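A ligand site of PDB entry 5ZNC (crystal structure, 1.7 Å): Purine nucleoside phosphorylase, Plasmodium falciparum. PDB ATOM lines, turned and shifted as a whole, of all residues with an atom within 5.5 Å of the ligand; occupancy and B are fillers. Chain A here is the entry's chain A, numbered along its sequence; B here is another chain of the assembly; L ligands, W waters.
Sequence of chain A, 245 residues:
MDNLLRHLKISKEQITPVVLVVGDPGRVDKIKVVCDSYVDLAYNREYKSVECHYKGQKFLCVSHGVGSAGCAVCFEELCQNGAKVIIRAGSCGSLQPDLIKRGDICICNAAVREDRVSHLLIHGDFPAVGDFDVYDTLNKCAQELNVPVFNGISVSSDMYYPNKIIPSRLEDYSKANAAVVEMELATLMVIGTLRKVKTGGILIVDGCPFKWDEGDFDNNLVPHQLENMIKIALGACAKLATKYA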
ATOM      1  N   VAL A  66       1.470  17.194 -16.902  1.00  0.00           N
ATOM      2  CA  VAL A  66       1.616  16.020 -17.704  1.00  0.00           C
ATOM      3  C   VAL A  66       3.057  15.626 -17.903  1.00  0.00           C
ATOM      4  O   VAL A  66       3.893  16.399 -18.466  1.00  0.00           O
ATOM      5  CB  VAL A  66       0.935  16.235 -19.060  1.00  0.00           C
ATOM      6  CG1 VAL A  66       1.095  14.992 -19.964  1.00  0.00           C
ATOM      7  CG2 VAL A  66      -0.540  16.559 -18.861  1.00  0.00           C
ATOM      8  N   ARG A  88      -0.378   9.732  -5.529  1.00  0.00           N
ATOM      9  CA  ARG A  88      -0.870  10.219  -6.779  1.00  0.00           C
ATOM     10  C   ARG A  88      -2.280   9.723  -7.068  1.00  0.00           C
ATOM     11  O   ARG A  88      -2.539   8.503  -6.996  1.00  0.00           O
ATOM     12  CB  ARG A  88       0.075   9.849  -7.948  1.00  0.00           C
ATOM     13  CG  ARG A  88      -0.453  10.058  -9.321  1.00  0.00           C
ATOM     14  CD  ARG A  88       0.643  10.023 -10.431  1.00  0.00           C
ATOM     15  NE  ARG A  88       0.079   9.521 -11.655  1.00  0.00           N
ATOM     16  CZ  ARG A  88      -0.809  10.155 -12.373  1.00  0.00           C
ATOM     17  NH1 ARG A  88      -1.177  11.404 -12.098  1.00  0.00           N
ATOM     18  NH2 ARG A  88      -1.379   9.522 -13.347  1.00  0.00           N
ATOM     19  N   SER A  91      -5.704   9.659 -13.812  1.00  0.00           N
ATOM     20  CA  SER A  91      -6.449   8.873 -14.757  1.00  0.00           C
ATOM     21  C   SER A  91      -5.499   7.912 -15.462  1.00  0.00           C
ATOM     22  O   SER A  91      -4.274   8.115 -15.462  1.00  0.00           O
ATOM     23  CB  SER A  91      -7.162   9.744 -15.701  1.00  0.00           C
ATOM     24  OG  SER A  91      -6.368  10.545 -16.543  1.00  0.00           O
ATOM     25  N   CYS A  92      -6.046   6.905 -16.145  1.00  0.00           N
ATOM     26  CA  CYS A  92      -5.194   5.933 -16.815  1.00  0.00           C
ATOM     27  C   CYS A  92      -6.047   5.255 -17.886  1.00  0.00           C
ATOM     28  O   CYS A  92      -7.288   5.408 -17.884  1.00  0.00           O
ATOM     29  CB  CYS A  92      -4.728   4.875 -15.869  1.00  0.00           C
ATOM     30  SG  CYS A  92      -6.076   3.784 -15.190  1.00  0.00           S
ATOM     31  N   GLY A  93      -5.364   4.486 -18.743  1.00  0.00           N
ATOM     32  CA  GLY A  93      -6.014   3.739 -19.800  1.00  0.00           C
ATOM     33  C   GLY A  93      -6.005   2.272 -19.464  1.00  0.00           C
ATOM     34  O   GLY A  93      -5.025   1.735 -18.956  1.00  0.00           O
ATOM     35  N   SER A 157       4.354   5.468 -19.222  1.00  0.00           N
ATOM     36  CA  SER A 157       5.044   5.708 -20.497  1.00  0.00           C
ATOM     37  C   SER A 157       5.114   7.184 -20.844  1.00  0.00           C
ATOM     38  O   SER A 157       4.109   7.921 -20.808  1.00  0.00           O
ATOM     39  CB  SER A 157       4.364   4.930 -21.662  1.00  0.00           C
ATOM     40  OG  SER A 157       5.003   5.232 -22.904  1.00  0.00           O
ATOM     41  N   ASP A 158       6.277   7.620 -21.279  1.00  0.00           N
ATOM     42  CA  ASP A 158       6.466   8.986 -21.767  1.00  0.00           C
ATOM     43  C   ASP A 158       5.893   9.230 -23.146  1.00  0.00           C
ATOM     44  O   ASP A 158       5.900  10.415 -23.563  1.00  0.00           O
ATOM     45  CB  ASP A 158       7.924   9.365 -21.795  1.00  0.00           C
ATOM     46  CG  ASP A 158       8.506   9.655 -20.458  1.00  0.00           C
ATOM     47  OD1 ASP A 158       7.921   9.439 -19.393  1.00  0.00           O
ATOM     48  OD2 ASP A 158       9.617  10.297 -20.434  1.00  0.00           O
ATOM     49  N   MET A 159       5.427   8.187 -23.846  1.00  0.00           N
ATOM     50  CA  MET A 159       4.847   8.403 -25.184  1.00  0.00           C
ATOM     51  C   MET A 159       3.307   8.178 -25.147  1.00  0.00           C
ATOM     52  O   MET A 159       2.820   7.076 -24.998  1.00  0.00           O
ATOM     53  CB  MET A 159       5.476   7.423 -26.170  1.00  0.00           C
ATOM     54  CG  MET A 159       4.911   7.596 -27.593  1.00  0.00           C
ATOM     55  SD  MET A 159       5.745   6.423 -28.713  1.00  0.00           S
ATOM     56  CE  MET A 159       5.193   4.834 -28.155  1.00  0.00           C
ATOM     57  N   TYR A 160       2.595   9.277 -25.336  1.00  0.00           N
ATOM     58  CA  TYR A 160       1.120   9.263 -25.423  1.00  0.00           C
ATOM     59  C   TYR A 160       0.693   8.928 -26.821  1.00  0.00           C
ATOM     60  O   TYR A 160      -0.192   8.076 -26.991  1.00  0.00           O
ATOM     61  CB  TYR A 160       0.595  10.591 -24.913  1.00  0.00           C
ATOM     62  CG  TYR A 160      -0.925  10.665 -24.959  1.00  0.00           C
ATOM     63  CD1 TYR A 160      -1.663   9.983 -24.013  1.00  0.00           C
ATOM     64  CD2 TYR A 160      -1.546  11.403 -25.937  1.00  0.00           C
ATOM     65  CE1 TYR A 160      -3.074  10.092 -23.989  1.00  0.00           C
ATOM     66  CE2 TYR A 160      -2.967  11.465 -25.969  1.00  0.00           C
ATOM     67  CZ  TYR A 160      -3.668  10.840 -24.970  1.00  0.00           C
ATOM     68  OH  TYR A 160      -5.083  10.927 -25.058  1.00  0.00           O
ATOM     69  N   LEU A 170       2.936  -1.338 -25.372  1.00  0.00           N
ATOM     70  CA  LEU A 170       1.705  -1.518 -24.590  1.00  0.00           C
ATOM     71  C   LEU A 170       1.171  -2.949 -24.699  1.00  0.00           C
ATOM     72  O   LEU A 170       0.762  -3.496 -23.682  1.00  0.00           O
ATOM     73  CB  LEU A 170       0.654  -0.473 -24.859  1.00  0.00           C
ATOM     74  CG  LEU A 170       0.936   0.970 -24.434  1.00  0.00           C
ATOM     75  CD1 LEU A 170      -0.196   1.900 -24.734  1.00  0.00           C
ATOM     76  CD2 LEU A 170       1.221   0.993 -22.991  1.00  0.00           C
ATOM     77  N   VAL A 181      -2.300   1.966 -18.022  1.00  0.00           N
ATOM     78  CA  VAL A 181      -1.225   2.841 -18.555  1.00  0.00           C
ATOM     79  C   VAL A 181      -1.481   4.275 -18.119  1.00  0.00           C
ATOM     80  O   VAL A 181      -2.567   4.789 -18.223  1.00  0.00           O
ATOM     81  CB  VAL A 181      -1.059   2.768 -20.075  1.00  0.00           C
ATOM     82  CG1 VAL A 181      -2.356   3.098 -20.879  1.00  0.00           C
ATOM     83  CG2 VAL A 181       0.042   3.730 -20.548  1.00  0.00           C
ATOM     84  N   GLU A 182      -0.431   4.942 -17.658  1.00  0.00           N
ATOM     85  CA  GLU A 182      -0.487   6.354 -17.361  1.00  0.00           C
ATOM     86  C   GLU A 182       0.935   6.963 -17.607  1.00  0.00           C
ATOM     87  O   GLU A 182       1.678   6.377 -18.322  1.00  0.00           O
ATOM     88  CB  GLU A 182      -1.156   6.745 -16.039  1.00  0.00           C
ATOM     89  CG  GLU A 182      -0.789   5.958 -14.834  1.00  0.00           C
ATOM     90  CD  GLU A 182       0.617   6.302 -14.349  1.00  0.00           C
ATOM     91  OE1 GLU A 182       1.479   5.433 -14.485  1.00  0.00           O
ATOM     92  OE2 GLU A 182       0.792   7.405 -13.867  1.00  0.00           O
ATOM     93  N   MET A 183       1.287   8.075 -16.939  1.00  0.00           N
ATOM     94  CA  MET A 183       2.509   8.755 -17.366  1.00  0.00           C
ATOM     95  C   MET A 183       3.434   9.166 -16.237  1.00  0.00           C
ATOM     96  O   MET A 183       4.487   9.723 -16.548  1.00  0.00           O
ATOM     97  CB  MET A 183       2.176  10.027 -18.222  1.00  0.00           C
ATOM     98  CG  MET A 183       1.427   9.646 -19.514  1.00  0.00           C
ATOM     99  SD  MET A 183       1.173  11.031 -20.641  1.00  0.00           S
ATOM    100  CE  MET A 183       2.814  11.338 -21.339  1.00  0.00           C
ATOM    101  N   GLU A 184       3.062   8.962 -14.994  1.00  0.00           N
ATOM    102  CA  GLU A 184       3.902   9.490 -13.878  1.00  0.00           C
ATOM    103  C   GLU A 184       4.219   8.591 -12.692  1.00  0.00           C
ATOM    104  O   GLU A 184       5.126   8.863 -11.859  1.00  0.00           O
ATOM    105  CB  GLU A 184       3.216  10.795 -13.373  1.00  0.00           C
ATOM    106  CG  GLU A 184       3.116  11.915 -14.373  1.00  0.00           C
ATOM    107  CD  GLU A 184       1.783  11.878 -15.130  1.00  0.00           C
ATOM    108  OE1 GLU A 184       0.887  11.035 -14.876  1.00  0.00           O
ATOM    109  OE2 GLU A 184       1.597  12.674 -16.041  1.00  0.00           O
ATOM    110  N   ASP A 206     -10.091   5.648 -18.000  1.00  0.00           N
ATOM    111  CA  ASP A 206     -10.656   6.515 -18.992  1.00  0.00           C
ATOM    112  C   ASP A 206     -10.236   6.022 -20.379  1.00  0.00           C
ATOM    113  O   ASP A 206      -9.273   6.456 -20.915  1.00  0.00           O
ATOM    114  CB  ASP A 206     -10.160   7.951 -18.717  1.00  0.00           C
ATOM    115  CG  ASP A 206     -10.958   9.031 -19.412  1.00  0.00           C
ATOM    116  OD1 ASP A 206     -11.903   8.736 -20.109  1.00  0.00           O
ATOM    117  OD2 ASP A 206     -10.568  10.189 -19.280  1.00  0.00           O
ATOM    118  N   GLY A 207     -10.973   5.073 -20.923  1.00  0.00           N
ATOM    119  CA  GLY A 207     -10.617   4.616 -22.214  1.00  0.00           C
ATOM    120  C   GLY A 207      -9.599   3.444 -22.201  1.00  0.00           C
ATOM    121  O   GLY A 207      -9.240   2.930 -21.158  1.00  0.00           O
ATOM    122  N   PRO A 209      -6.315   2.429 -24.823  1.00  0.00           N
ATOM    123  CA  PRO A 209      -5.547   2.755 -25.981  1.00  0.00           C
ATOM    124  C   PRO A 209      -5.681   1.774 -27.195  1.00  0.00           C
ATOM    125  O   PRO A 209      -5.470   2.158 -28.296  1.00  0.00           O
ATOM    126  CB  PRO A 209      -4.072   2.798 -25.445  1.00  0.00           C
ATOM    127  CG  PRO A 209      -4.126   2.088 -24.198  1.00  0.00           C
ATOM    128  CD  PRO A 209      -5.505   2.274 -23.600  1.00  0.00           C
ATOM    129  N   TRP A 212      -8.607   3.117 -29.352  1.00  0.00           N
ATOM    130  CA  TRP A 212      -8.711   4.480 -29.808  1.00  0.00           C
ATOM    131  C   TRP A 212      -9.184   4.616 -31.278  1.00  0.00           C
ATOM    132  O   TRP A 212      -9.808   5.602 -31.620  1.00  0.00           O
ATOM    133  CB  TRP A 212      -7.406   5.225 -29.660  1.00  0.00           C
ATOM    134  CG  TRP A 212      -7.038   5.635 -28.260  1.00  0.00           C
ATOM    135  CD1 TRP A 212      -7.691   5.440 -27.118  1.00  0.00           C
ATOM    136  CD2 TRP A 212      -5.814   6.327 -27.926  1.00  0.00           C
ATOM    137  NE1 TRP A 212      -6.970   6.062 -26.061  1.00  0.00           N
ATOM    138  CE2 TRP A 212      -5.819   6.566 -26.574  1.00  0.00           C
ATOM    139  CE3 TRP A 212      -4.760   6.779 -28.684  1.00  0.00           C
ATOM    140  CZ2 TRP A 212      -4.773   7.276 -25.926  1.00  0.00           C
ATOM    141  CZ3 TRP A 212      -3.691   7.461 -28.061  1.00  0.00           C
ATOM    142  CH2 TRP A 212      -3.750   7.699 -26.715  1.00  0.00           C
ATOM    143  N   ASP A 218      -9.473   8.810 -23.838  1.00  0.00           N
ATOM    144  CA  ASP A 218      -9.490   9.271 -22.501  1.00  0.00           C
ATOM    145  C   ASP A 218     -10.164  10.644 -22.486  1.00  0.00           C
ATOM    146  O   ASP A 218      -9.493  11.656 -22.457  1.00  0.00           O
ATOM    147  CB  ASP A 218      -8.088   9.315 -21.920  1.00  0.00           C
ATOM    148  CG  ASP A 218      -7.057   9.759 -22.842  1.00  0.00           C
ATOM    149  OD1 ASP A 218      -7.153   9.682 -23.992  1.00  0.00           O
ATOM    150  OD2 ASP A 218      -6.031  10.129 -22.394  1.00  0.00           O
ATOM    151  N   HIS B   7      -6.297  17.360 -26.453  1.00  0.00           N
ATOM    152  CA  HIS B   7      -5.830  17.952 -25.179  1.00  0.00           C
ATOM    153  C   HIS B   7      -5.544  19.456 -25.200  1.00  0.00           C
ATOM    154  O   HIS B   7      -5.610  20.141 -24.144  1.00  0.00           O
ATOM    155  CB  HIS B   7      -4.673  17.095 -24.598  1.00  0.00           C
ATOM    156  CG  HIS B   7      -5.096  15.676 -24.417  1.00  0.00           C
ATOM    157  ND1 HIS B   7      -5.999  15.292 -23.446  1.00  0.00           N
ATOM    158  CD2 HIS B   7      -4.743  14.557 -25.078  1.00  0.00           C
ATOM    159  CE1 HIS B   7      -6.211  13.986 -23.583  1.00  0.00           C
ATOM    160  NE2 HIS B   7      -5.483  13.516 -24.580  1.00  0.00           N
ATOM    161  N   ARG B  45      -5.358  22.382 -18.720  1.00  0.00           N
ATOM    162  CA  ARG B  45      -4.165  21.881 -18.016  1.00  0.00           C
ATOM    163  C   ARG B  45      -3.077  22.965 -18.102  1.00  0.00           C
ATOM    164  O   ARG B  45      -3.394  24.129 -17.927  1.00  0.00           O
ATOM    165  CB  ARG B  45      -3.729  20.520 -18.632  1.00  0.00           C
ATOM    166  CG  ARG B  45      -4.737  19.440 -18.348  1.00  0.00           C
ATOM    167  CD  ARG B  45      -4.391  18.116 -19.033  1.00  0.00           C
ATOM    168  NE  ARG B  45      -5.251  17.021 -18.563  1.00  0.00           N
ATOM    169  CZ  ARG B  45      -4.997  16.244 -17.529  1.00  0.00           C
ATOM    170  NH1 ARG B  45      -3.863  16.364 -16.832  1.00  0.00           N
ATOM    171  NH2 ARG B  45      -5.859  15.278 -17.186  1.00  0.00           N
ATOM    172  N   TYR B  47      -1.646  23.813 -20.906  1.00  0.00           N
ATOM    173  CA  TYR B  47      -1.644  24.199 -22.311  1.00  0.00           C
ATOM    174  C   TYR B  47      -2.581  25.442 -22.586  1.00  0.00           C
ATOM    175  O   TYR B  47      -3.803  25.272 -22.657  1.00  0.00           O
ATOM    176  CB  TYR B  47      -2.105  23.018 -23.172  1.00  0.00           C
ATOM    177  CG  TYR B  47      -1.360  21.741 -22.890  1.00  0.00           C
ATOM    178  CD1 TYR B  47      -0.010  21.584 -23.155  1.00  0.00           C
ATOM    179  CD2 TYR B  47      -2.018  20.620 -22.415  1.00  0.00           C
ATOM    180  CE1 TYR B  47       0.676  20.398 -22.962  1.00  0.00           C
ATOM    181  CE2 TYR B  47      -1.333  19.435 -22.157  1.00  0.00           C
ATOM    182  CZ  TYR B  47       0.018  19.304 -22.456  1.00  0.00           C
ATOM    183  OH  TYR B  47       0.643  18.095 -22.199  1.00  0.00           O
ATOM    184  N   VAL B  73       2.879  15.846 -26.150  1.00  0.00           N
ATOM    185  CA  VAL B  73       1.418  15.831 -26.396  1.00  0.00           C
ATOM    186  C   VAL B  73       1.036  17.078 -27.217  1.00  0.00           C
ATOM    187  O   VAL B  73       0.346  17.005 -28.219  1.00  0.00           O
ATOM    188  CB  VAL B  73       0.653  15.749 -25.107  1.00  0.00           C
ATOM    189  CG1 VAL B  73      -0.835  15.819 -25.362  1.00  0.00           C
ATOM    190  CG2 VAL B  73       0.998  14.446 -24.389  1.00  0.00           C
HETATM  191  O1  LIG L   1      -1.714   9.014 -18.696  1.00  0.00           O
HETATM  192  C1  LIG L   1      -3.016   9.445 -19.122  1.00  0.00           C
HETATM  193  C2  LIG L   1      -2.871  10.675 -20.072  1.00  0.00           C
HETATM  194  N1  LIG L   1      -4.208  11.129 -20.653  1.00  0.00           N
HETATM  195  C3  LIG L   1      -5.085  11.581 -19.547  1.00  0.00           C
HETATM  196  C4  LIG L   1      -4.309  12.497 -18.557  1.00  0.00           C
HETATM  197  C5  LIG L   1      -3.906  12.300 -21.495  1.00  0.00           C
HETATM  198  C6  LIG L   1      -3.563  13.561 -20.654  1.00  0.00           C
HETATM  199  C7  LIG L   1      -2.572  14.470 -21.344  1.00  0.00           C
HETATM  200  C8  LIG L   1      -2.812  15.693 -21.724  1.00  0.00           C
HETATM  201  C9  LIG L   1      -3.091  13.044 -19.282  1.00  0.00           C
HETATM  202  C10 LIG L   1      -2.104  11.878 -19.464  1.00  0.00           C
HETATM  203  C11 LIG L   1      -3.782   8.339 -19.858  1.00  0.00           C
HETATM  204  C12 LIG L   1      -5.106   8.163 -19.557  1.00  0.00           C
HETATM  205  C13 LIG L   1      -5.891   7.296 -20.325  1.00  0.00           C
HETATM  206  N2  LIG L   1      -5.430   6.601 -21.356  1.00  0.00           N
HETATM  207  C14 LIG L   1      -4.112   6.726 -21.683  1.00  0.00           C
HETATM  208  C15 LIG L   1      -3.238   7.569 -20.948  1.00  0.00           C
HETATM  209  C16 LIG L   1      -1.876   7.625 -21.328  1.00  0.00           C
HETATM  210  C17 LIG L   1      -3.620   5.960 -22.750  1.00  0.00           C
HETATM  211  C18 LIG L   1      -2.312   6.042 -23.105  1.00  0.00           C
HETATM  212  C19 LIG L   1      -1.412   6.798 -22.310  1.00  0.00           C
HETATM  213  O2  LIG L   1      -0.137   6.731 -22.807  1.00  0.00           O
HETATM  214  C20 LIG L   1       0.898   7.332 -22.015  1.00  0.00           C
HETATM  215  O   HOH W   1      -8.055  12.974 -20.465  1.00  0.00           O
HETATM  216  O   HOH W   2      -7.279   5.726 -23.308  1.00  0.00           O
HETATM  217  O   HOH W   3      -1.202  10.419 -16.504  1.00  0.00           O
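The backbone NH of Gly 93 lies close to a nitrogen (N2) of the ligand. A nitrogen (N1) of the ligand is in salt-bridge range of the side-chain carboxylate of Asp 218.
Water W3 lies within hydrogen-bond range of an oxygen (O1) of the ligand (2.7 Å), the side-chain carboxylate (OE1) of Glu 184 (2.7 Å), the guanidinium group (NH2) of Arg 88 (3.3 Å) and the backbone NH (N) of Met 183 (3.4 Å). Water W2 lies within hydrogen-bond range of the indole nitrogen of Trp 212 (2.8 Å), a nitrogen (N2) of the ligand (2.8 Å) and the backbone carbonyl oxygen of Asp 206 (3.2 Å).
Val 66 touches the ligand. Ser 91 touches the ligand. Cys 92 touches the ligand. Ser 157 touches the ligand. Met 159 touches the ligand (O to C20, 3.6 Å). CE1 of Tyr 160 touches C5 of the ligand, at 3.4 Å. Val 181 touches the ligand (CG1 to C17, 3.6 Å). Glu 182 touches the ligand (CA to O1, 3.2 Å). Met 183 touches the ligand. O of Asp 206 touches C13 of the ligand, at 3.5 Å. Trp 212 touches the ligand. CG of His 7 of chain B touches C8 of the ligand, at 3.5 Å. NH2 of Arg 45 of chain B touches C4 of the ligand, 3.5 Å away. Hydrophobic or aromatic side chains that line the ligand: Val 66, Tyr 160, Val 181, Met 183, Trp 212 and His 7 of chain B.
The guanidinium group (NH2) of Arg 88 is in salt-bridge range of the side-chain carboxylate (OE2) of Glu 182 (3.1 Å). N of Gly 93 lies within hydrogen-bond range of O of Val 181 (2.9 Å). OE2 of Glu 182 sits at hydrogen-bond distance from N of Glu 184 (3.0 Å). The backbone NH (N) of Met 159 sits at hydrogen-bond distance from the side-chain hydroxyl (OG) of Ser 157 (3.1 Å). The side-chain carboxylate (OD1) of Asp 218 is in hydrogen-bond range of the side-chain hydroxyl (OH) of Tyr 160, at 2.6 Å. The backbone NH of Ser 157 sits at hydrogen-bond distance from the backbone carbonyl oxygen of Glu 182, at 3.0 Å. The backbone carbonyl oxygen (O) of Cys 92 sits at hydrogen-bond distance from the backbone NH (N) of Asp 206 (2.8 Å). The side-chain hydroxyl of Tyr 160 sits at hydrogen-bond distance from a ring nitrogen (NE2) of His 7 of chain B, 2.7 Å away.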
